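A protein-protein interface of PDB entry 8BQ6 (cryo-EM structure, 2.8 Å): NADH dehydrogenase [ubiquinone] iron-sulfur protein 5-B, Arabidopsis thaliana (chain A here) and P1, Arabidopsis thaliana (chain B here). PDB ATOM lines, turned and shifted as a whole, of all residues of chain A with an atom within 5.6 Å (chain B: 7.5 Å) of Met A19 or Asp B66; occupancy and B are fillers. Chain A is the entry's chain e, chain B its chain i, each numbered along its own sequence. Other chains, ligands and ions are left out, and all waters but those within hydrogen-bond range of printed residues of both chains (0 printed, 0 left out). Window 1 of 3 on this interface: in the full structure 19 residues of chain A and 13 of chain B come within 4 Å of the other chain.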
ATOM      1  N   ALA A   2      32.494  21.561   4.707  1.00  0.00           N
ATOM      2  CA  ALA A   2      31.725  20.344   4.370  1.00  0.00           C
ATOM      3  C   ALA A   2      30.250  20.696   4.178  1.00  0.00           C
ATOM      4  O   ALA A   2      29.522  19.843   3.669  1.00  0.00           O
ATOM      5  CB  ALA A   2      31.901  19.322   5.459  1.00  0.00           C
ATOM      6  N   SER A   3      29.831  21.900   4.576  1.00  0.00           N
ATOM      7  CA  SER A   3      28.393  22.276   4.520  1.00  0.00           C
ATOM      8  C   SER A   3      27.981  22.718   3.115  1.00  0.00           C
ATOM      9  O   SER A   3      26.830  22.489   2.768  1.00  0.00           O
ATOM     10  CB  SER A   3      28.063  23.324   5.549  1.00  0.00           C
ATOM     11  OG  SER A   3      28.304  24.638   5.066  1.00  0.00           O
ATOM     12  N   CYS A  14      35.982  24.180  -0.772  1.00  0.00           N
ATOM     13  CA  CYS A  14      36.370  22.794  -0.551  1.00  0.00           C
ATOM     14  C   CYS A  14      35.186  21.834  -0.516  1.00  0.00           C
ATOM     15  O   CYS A  14      35.326  20.714  -0.018  1.00  0.00           O
ATOM     16  CB  CYS A  14      37.176  22.682   0.742  1.00  0.00           C
ATOM     17  SG  CYS A  14      38.666  23.711   0.764  1.00  0.00           S
ATOM     18  N   TYR A  15      34.026  22.251  -1.021  1.00  0.00           N
ATOM     19  CA  TYR A  15      32.803  21.412  -0.950  1.00  0.00           C
ATOM     20  C   TYR A  15      32.898  20.239  -1.923  1.00  0.00           C
ATOM     21  O   TYR A  15      32.508  19.135  -1.550  1.00  0.00           O
ATOM     22  CB  TYR A  15      31.570  22.236  -1.304  1.00  0.00           C
ATOM     23  CG  TYR A  15      30.269  21.485  -1.318  1.00  0.00           C
ATOM     24  CD1 TYR A  15      29.804  20.816  -0.199  1.00  0.00           C
ATOM     25  CD2 TYR A  15      29.498  21.455  -2.465  1.00  0.00           C
ATOM     26  CE1 TYR A  15      28.597  20.141  -0.220  1.00  0.00           C
ATOM     27  CE2 TYR A  15      28.293  20.783  -2.508  1.00  0.00           C
ATOM     28  CZ  TYR A  15      27.845  20.125  -1.381  1.00  0.00           C
ATOM     29  OH  TYR A  15      26.657  19.469  -1.447  1.00  0.00           O
ATOM     30  N   ASP A  16      33.382  20.487  -3.136  1.00  0.00           N
ATOM     31  CA  ASP A  16      33.445  19.411  -4.122  1.00  0.00           C
ATOM     32  C   ASP A  16      34.376  18.291  -3.667  1.00  0.00           C
ATOM     33  O   ASP A  16      34.074  17.108  -3.864  1.00  0.00           O
ATOM     34  CB  ASP A  16      33.882  19.966  -5.474  1.00  0.00           C
ATOM     35  CG  ASP A  16      32.773  20.725  -6.173  1.00  0.00           C
ATOM     36  OD1 ASP A  16      31.596  20.526  -5.809  1.00  0.00           O
ATOM     37  OD2 ASP A  16      33.071  21.532  -7.077  1.00  0.00           O
ATOM     38  N   PHE A  17      35.508  18.644  -3.055  1.00  0.00           N
ATOM     39  CA  PHE A  17      36.397  17.630  -2.495  1.00  0.00           C
ATOM     40  C   PHE A  17      35.703  16.848  -1.389  1.00  0.00           C
ATOM     41  O   PHE A  17      35.841  15.620  -1.292  1.00  0.00           O
ATOM     42  CB  PHE A  17      37.672  18.278  -1.956  1.00  0.00           C
ATOM     43  CG  PHE A  17      38.640  18.703  -3.019  1.00  0.00           C
ATOM     44  CD1 PHE A  17      39.324  17.759  -3.765  1.00  0.00           C
ATOM     45  CD2 PHE A  17      38.903  20.043  -3.243  1.00  0.00           C
ATOM     46  CE1 PHE A  17      40.224  18.144  -4.735  1.00  0.00           C
ATOM     47  CE2 PHE A  17      39.808  20.433  -4.209  1.00  0.00           C
ATOM     48  CZ  PHE A  17      40.467  19.483  -4.956  1.00  0.00           C
ATOM     49  N   TRP A  18      34.982  17.562  -0.522  1.00  0.00           N
ATOM     50  CA  TRP A  18      34.232  16.889   0.568  1.00  0.00           C
ATOM     51  C   TRP A  18      33.240  15.900  -0.038  1.00  0.00           C
ATOM     52  O   TRP A  18      33.184  14.767   0.438  1.00  0.00           O
ATOM     53  CB  TRP A  18      33.504  17.904   1.460  1.00  0.00           C
ATOM     54  CG  TRP A  18      32.519  17.226   2.356  1.00  0.00           C
ATOM     55  CD1 TRP A  18      31.159  17.266   2.278  1.00  0.00           C
ATOM     56  CD2 TRP A  18      32.837  16.326   3.428  1.00  0.00           C
ATOM     57  NE1 TRP A  18      30.609  16.473   3.245  1.00  0.00           N
ATOM     58  CE2 TRP A  18      31.612  15.885   3.967  1.00  0.00           C
ATOM     59  CE3 TRP A  18      34.029  15.865   3.990  1.00  0.00           C
ATOM     60  CZ2 TRP A  18      31.552  15.006   5.044  1.00  0.00           C
ATOM     61  CZ3 TRP A  18      33.965  14.991   5.048  1.00  0.00           C
ATOM     62  CH2 TRP A  18      32.744  14.571   5.569  1.00  0.00           C
ATOM     63  N   MET A  19      32.485  16.337  -1.046  1.00  0.00           N
ATOM     64  CA  MET A  19      31.470  15.474  -1.633  1.00  0.00           C
ATOM     65  C   MET A  19      32.093  14.266  -2.322  1.00  0.00           C
ATOM     66  O   MET A  19      31.540  13.163  -2.258  1.00  0.00           O
ATOM     67  CB  MET A  19      30.599  16.267  -2.602  1.00  0.00           C
ATOM     68  CG  MET A  19      29.602  17.159  -1.901  1.00  0.00           C
ATOM     69  SD  MET A  19      28.915  16.354  -0.440  1.00  0.00           S
ATOM     70  CE  MET A  19      27.188  16.251  -0.889  1.00  0.00           C
ATOM     71  N   ASP A  20      33.240  14.445  -2.981  1.00  0.00           N
ATOM     72  CA  ASP A  20      33.943  13.295  -3.547  1.00  0.00           C
ATOM     73  C   ASP A  20      34.327  12.301  -2.460  1.00  0.00           C
ATOM     74  O   ASP A  20      34.099  11.091  -2.595  1.00  0.00           O
ATOM     75  CB  ASP A  20      35.188  13.752  -4.301  1.00  0.00           C
ATOM     76  CG  ASP A  20      34.862  14.610  -5.492  1.00  0.00           C
ATOM     77  OD1 ASP A  20      35.770  15.308  -5.984  1.00  0.00           O
ATOM     78  OD2 ASP A  20      33.698  14.580  -5.943  1.00  0.00           O
ATOM     79  N   PHE A  21      34.906  12.799  -1.367  1.00  0.00           N
ATOM     80  CA  PHE A  21      35.312  11.913  -0.282  1.00  0.00           C
ATOM     81  C   PHE A  21      34.111  11.196   0.327  1.00  0.00           C
ATOM     82  O   PHE A  21      34.172   9.994   0.616  1.00  0.00           O
ATOM     83  CB  PHE A  21      36.065  12.716   0.774  1.00  0.00           C
ATOM     84  CG  PHE A  21      36.333  11.962   2.037  1.00  0.00           C
ATOM     85  CD1 PHE A  21      37.107  10.822   2.026  1.00  0.00           C
ATOM     86  CD2 PHE A  21      35.819  12.406   3.241  1.00  0.00           C
ATOM     87  CE1 PHE A  21      37.357  10.135   3.191  1.00  0.00           C
ATOM     88  CE2 PHE A  21      36.066  11.723   4.406  1.00  0.00           C
ATOM     89  CZ  PHE A  21      36.837  10.588   4.382  1.00  0.00           C
ATOM     90  N   SER A  22      33.004  11.916   0.515  1.00  0.00           N
ATOM     91  CA  SER A  22      31.816  11.315   1.112  1.00  0.00           C
ATOM     92  C   SER A  22      31.214  10.255   0.203  1.00  0.00           C
ATOM     93  O   SER A  22      30.847   9.166   0.663  1.00  0.00           O
ATOM     94  CB  SER A  22      30.781  12.394   1.420  1.00  0.00           C
ATOM     95  OG  SER A  22      31.265  13.280   2.408  1.00  0.00           O
ATOM     96  N   GLU A  23      31.089  10.559  -1.088  1.00  0.00           N
ATOM     97  CA  GLU A  23      30.526   9.589  -2.014  1.00  0.00           C
ATOM     98  C   GLU A  23      31.407   8.348  -2.098  1.00  0.00           C
ATOM     99  O   GLU A  23      30.897   7.224  -2.160  1.00  0.00           O
ATOM    100  CB  GLU A  23      30.328  10.227  -3.390  1.00  0.00           C
ATOM    101  CG  GLU A  23      29.218  11.247  -3.461  1.00  0.00           C
ATOM    102  CD  GLU A  23      29.020  11.831  -4.832  1.00  0.00           C
ATOM    103  OE1 GLU A  23      28.286  11.211  -5.628  1.00  0.00           O
ATOM    104  OE2 GLU A  23      29.590  12.904  -5.119  1.00  0.00           O
ATOM    105  N   CYS A  24      32.732   8.522  -2.065  1.00  0.00           N
ATOM    106  CA  CYS A  24      33.608   7.353  -2.016  1.00  0.00           C
ATOM    107  C   CYS A  24      33.370   6.541  -0.748  1.00  0.00           C
ATOM    108  O   CYS A  24      33.263   5.311  -0.800  1.00  0.00           O
ATOM    109  CB  CYS A  24      35.077   7.772  -2.114  1.00  0.00           C
ATOM    110  SG  CYS A  24      36.276   6.392  -2.051  1.00  0.00           S
ATOM    111  N   ALA B  61      22.906  10.760   4.960  1.00  0.00           N
ATOM    112  CA  ALA B  61      21.821  11.721   4.798  1.00  0.00           C
ATOM    113  C   ALA B  61      22.238  12.894   3.914  1.00  0.00           C
ATOM    114  O   ALA B  61      21.455  13.351   3.074  1.00  0.00           O
ATOM    115  CB  ALA B  61      21.350  12.211   6.166  1.00  0.00           C
ATOM    116  N   GLN B  62      23.452  13.408   4.115  1.00  0.00           N
ATOM    117  CA  GLN B  62      23.934  14.581   3.336  1.00  0.00           C
ATOM    118  C   GLN B  62      23.965  14.258   1.836  1.00  0.00           C
ATOM    119  O   GLN B  62      23.573  15.120   1.048  1.00  0.00           O
ATOM    120  CB  GLN B  62      25.313  14.993   3.852  1.00  0.00           C
ATOM    121  CG  GLN B  62      26.011  16.032   2.985  1.00  0.00           C
ATOM    122  CD  GLN B  62      27.140  16.742   3.687  1.00  0.00           C
ATOM    123  OE1 GLN B  62      27.831  16.174   4.526  1.00  0.00           O
ATOM    124  NE2 GLN B  62      27.343  17.999   3.334  1.00  0.00           N
ATOM    125  N   LEU B  63      24.374  13.044   1.462  1.00  0.00           N
ATOM    126  CA  LEU B  63      24.508  12.690   0.054  1.00  0.00           C
ATOM    127  C   LEU B  63      23.174  12.682  -0.681  1.00  0.00           C
ATOM    128  O   LEU B  63      23.160  12.756  -1.914  1.00  0.00           O
ATOM    129  CB  LEU B  63      25.175  11.325  -0.076  1.00  0.00           C
ATOM    130  CG  LEU B  63      26.695  11.364   0.052  1.00  0.00           C
ATOM    131  CD1 LEU B  63      27.254   9.969   0.236  1.00  0.00           C
ATOM    132  CD2 LEU B  63      27.294  12.057  -1.134  1.00  0.00           C
ATOM    133  N   ARG B  64      22.059  12.585   0.037  1.00  0.00           N
ATOM    134  CA  ARG B  64      20.754  12.603  -0.603  1.00  0.00           C
ATOM    135  C   ARG B  64      20.017  13.919  -0.419  1.00  0.00           C
ATOM    136  O   ARG B  64      19.140  14.238  -1.227  1.00  0.00           O
ATOM    137  CB  ARG B  64      19.889  11.455  -0.073  1.00  0.00           C
ATOM    138  CG  ARG B  64      20.693  10.215   0.255  1.00  0.00           C
ATOM    139  CD  ARG B  64      19.865   8.957   0.077  1.00  0.00           C
ATOM    140  NE  ARG B  64      18.781   8.850   1.046  1.00  0.00           N
ATOM    141  CZ  ARG B  64      18.943   8.507   2.317  1.00  0.00           C
ATOM    142  NH1 ARG B  64      20.138   8.230   2.812  1.00  0.00           N
ATOM    143  NH2 ARG B  64      17.877   8.437   3.110  1.00  0.00           N
ATOM    144  N   TRP B  65      20.366  14.693   0.607  1.00  0.00           N
ATOM    145  CA  TRP B  65      19.690  15.960   0.841  1.00  0.00           C
ATOM    146  C   TRP B  65      20.382  17.099   0.104  1.00  0.00           C
ATOM    147  O   TRP B  65      19.719  17.945  -0.504  1.00  0.00           O
ATOM    148  CB  TRP B  65      19.619  16.242   2.341  1.00  0.00           C
ATOM    149  CG  TRP B  65      19.190  17.628   2.668  1.00  0.00           C
ATOM    150  CD1 TRP B  65      19.980  18.643   3.109  1.00  0.00           C
ATOM    151  CD2 TRP B  65      17.864  18.158   2.584  1.00  0.00           C
ATOM    152  NE1 TRP B  65      19.232  19.775   3.305  1.00  0.00           N
ATOM    153  CE2 TRP B  65      17.927  19.503   2.989  1.00  0.00           C
ATOM    154  CE3 TRP B  65      16.630  17.628   2.197  1.00  0.00           C
ATOM    155  CZ2 TRP B  65      16.807  20.324   3.022  1.00  0.00           C
ATOM    156  CZ3 TRP B  65      15.519  18.445   2.231  1.00  0.00           C
ATOM    157  CH2 TRP B  65      15.614  19.776   2.640  1.00  0.00           C
ATOM    158  N   ASP B  66      21.713  17.129   0.135  1.00  0.00           N
ATOM    159  CA  ASP B  66      22.449  18.185  -0.557  1.00  0.00           C
ATOM    160  C   ASP B  66      22.119  18.309  -2.041  1.00  0.00           C
ATOM    161  O   ASP B  66      22.031  19.450  -2.524  1.00  0.00           O
ATOM    162  CB  ASP B  66      23.958  17.997  -0.346  1.00  0.00           C
ATOM    163  CG  ASP B  66      24.475  18.776   0.850  1.00  0.00           C
ATOM    164  OD1 ASP B  66      23.647  19.378   1.566  1.00  0.00           O
ATOM    165  OD2 ASP B  66      25.702  18.798   1.072  1.00  0.00           O
ATOM    166  N   PRO B  67      21.950  17.230  -2.818  1.00  0.00           N
ATOM    167  CA  PRO B  67      21.516  17.417  -4.215  1.00  0.00           C
ATOM    168  C   PRO B  67      20.180  18.126  -4.351  1.00  0.00           C
ATOM    169  O   PRO B  67      19.958  18.816  -5.354  1.00  0.00           O
ATOM    170  CB  PRO B  67      21.448  15.988  -4.771  1.00  0.00           C
ATOM    171  CG  PRO B  67      22.185  15.144  -3.837  1.00  0.00           C
ATOM    172  CD  PRO B  67      22.321  15.833  -2.529  1.00  0.00           C
ATOM    173  N   GLN B  68      19.277  17.970  -3.381  1.00  0.00           N
ATOM    174  CA  GLN B  68      17.979  18.628  -3.451  1.00  0.00           C
ATOM    175  C   GLN B  68      18.078  20.138  -3.256  1.00  0.00           C
ATOM    176  O   GLN B  68      17.188  20.864  -3.709  1.00  0.00           O
ATOM    177  CB  GLN B  68      17.035  18.029  -2.410  1.00  0.00           C
ATOM    178  CG  GLN B  68      16.649  16.589  -2.675  1.00  0.00           C
ATOM    179  CD  GLN B  68      15.865  15.990  -1.532  1.00  0.00           C
ATOM    180  OE1 GLN B  68      14.780  16.462  -1.198  1.00  0.00           O
ATOM    181  NE2 GLN B  68      16.414  14.952  -0.915  1.00  0.00           N
ATOM    182  N   ILE B  69      19.124  20.627  -2.594  1.00  0.00           N
ATOM    183  CA  ILE B  69      19.333  22.058  -2.417  1.00  0.00           C
ATOM    184  C   ILE B  69      20.480  22.565  -3.288  1.00  0.00           C
ATOM    185  O   ILE B  69      20.968  23.671  -3.078  1.00  0.00           O
ATOM    186  CB  ILE B  69      19.579  22.421  -0.943  1.00  0.00           C
ATOM    187  CG1 ILE B  69      20.555  21.427  -0.306  1.00  0.00           C
ATOM    188  CG2 ILE B  69      18.263  22.523  -0.183  1.00  0.00           C
ATOM    189  CD1 ILE B  69      21.160  21.901   0.984  1.00  0.00           C
ATOM    190  N   SER B  70      20.919  21.771  -4.265  1.00  0.00           N
ATOM    191  CA  SER B  70      22.111  22.123  -5.028  1.00  0.00           C
ATOM    192  C   SER B  70      21.917  23.358  -5.899  1.00  0.00           C
ATOM    193  O   SER B  70      22.907  23.910  -6.391  1.00  0.00           O
ATOM    194  CB  SER B  70      22.548  20.937  -5.888  1.00  0.00           C
ATOM    195  OG  SER B  70      21.600  20.660  -6.902  1.00  0.00           O
ATOM    196  N   GLN B  71      20.676  23.805  -6.096  1.00  0.00           N
ATOM    197  CA  GLN B  71      20.361  24.972  -6.910  1.00  0.00           C
ATOM    198  C   GLN B  71      19.991  26.196  -6.080  1.00  0.00           C
ATOM    199  O   GLN B  71      19.536  27.196  -6.642  1.00  0.00           O
ATOM    200  CB  GLN B  71      19.216  24.647  -7.870  1.00  0.00           C
ATOM    201  CG  GLN B  71      19.633  24.375  -9.296  1.00  0.00           C
ATOM    202  CD  GLN B  71      20.876  23.526  -9.387  1.00  0.00           C
ATOM    203  OE1 GLN B  71      21.969  24.029  -9.638  1.00  0.00           O
ATOM    204  NE2 GLN B  71      20.719  22.226  -9.174  1.00  0.00           N
ATOM    205  N   VAL B  72      20.174  26.140  -4.766  1.00  0.00           N
ATOM    206  CA  VAL B  72      19.713  27.196  -3.870  1.00  0.00           C
ATOM    207  C   VAL B  72      20.739  28.321  -3.833  1.00  0.00           C
ATOM    208  O   VAL B  72      21.946  28.073  -3.716  1.00  0.00           O
ATOM    209  CB  VAL B  72      19.457  26.627  -2.466  1.00  0.00           C
ATOM    210  CG1 VAL B  72      19.383  27.734  -1.444  1.00  0.00           C
ATOM    211  CG2 VAL B  72      18.179  25.806  -2.456  1.00  0.00           C
ATOM    212  N   ARG B  75      24.759  28.622  -2.344  1.00  0.00           N
ATOM    213  CA  ARG B  75      25.664  27.482  -2.456  1.00  0.00           C
ATOM    214  C   ARG B  75      25.841  27.005  -3.895  1.00  0.00           C
ATOM    215  O   ARG B  75      26.225  25.848  -4.108  1.00  0.00           O
ATOM    216  CB  ARG B  75      25.193  26.316  -1.577  1.00  0.00           C
ATOM    217  CG  ARG B  75      23.805  25.781  -1.867  1.00  0.00           C
ATOM    218  CD  ARG B  75      23.405  24.760  -0.813  1.00  0.00           C
ATOM    219  NE  ARG B  75      24.233  23.560  -0.849  1.00  0.00           N
ATOM    220  CZ  ARG B  75      24.875  23.057   0.197  1.00  0.00           C
ATOM    221  NH1 ARG B  75      24.854  23.656   1.375  1.00  0.00           N
ATOM    222  NH2 ARG B  75      25.562  21.928   0.054  1.00  0.00           N
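Among the printed residues, pairs that only touch across the chains: Met A19 with Asp B66 (3.5 Å), Ser A22 with Leu B63 (3.7 Å) and Glu A23 with Leu B63 (3.1 Å).
Printed residues of chain B within 4 Å of Met A19: Asp B66.
Asp B66 touches two residues of chain A.
Printed residues of chain A within 4 Å of Arg B75: Ser A3 (2.7 Å) and Tyr A15 (3.1 Å).
Of the printed residues of chain B, Trp A18 touches Gln B62 (3.1 Å).
Of the printed residues of chain B, Ser A3 touches Arg B75 (2.7 Å).
The backbone carbonyl oxygen (O) of Ala A2 is in hydrogen-bond range of the side-chain amide nitrogen (NE2) of Gln B62, at 2.9 Å.
The guanidinium group (NH1) of Arg B75 sits at hydrogen-bond distance from the backbone carbonyl oxygen (O) of Ser A3.
The side-chain hydroxyl of Tyr A15 lies within hydrogen-bond range of the side-chain carboxylate of Asp B66 (2.8 Å).
OH of Tyr A15 lies within hydrogen-bond range of NH2 of Arg B75.
NE1 of Trp A18 is in hydrogen-bond range of OE1 of Gln B62, 3.1 Å away.
The backbone carbonyl oxygen (O) of Trp A18 lies close to the side-chain hydroxyl (OG) of Ser A22, at 3.1 Å.
The side-chain amide nitrogen of Gln B62 is in hydrogen-bond range of the side-chain carboxylate of Asp B66.
The side-chain carboxylate (OD2) of Asp B66 lies within salt-bridge range of the guanidinium group (NH2) of Arg B75 (3.3 Å).
Printed residues of chain A that touch a printed residue of chain B: Ala A2, Ser A3, Tyr A15, Trp A18, Met A19, Ser A22 and Glu A23.
Hydrophobic or aromatic side chains of chain A that line the printed part of chain B: Tyr A15, Trp A18 and Met A19.
Printed residues of chain B that touch a printed residue of chain A: Gln B62, Leu B63, Asp B66 and Arg B75.
Among the printed residues, no Asp or Glu carboxylate lies within 4 Å of a Lys or Arg side-chain nitrogen of the other chain.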
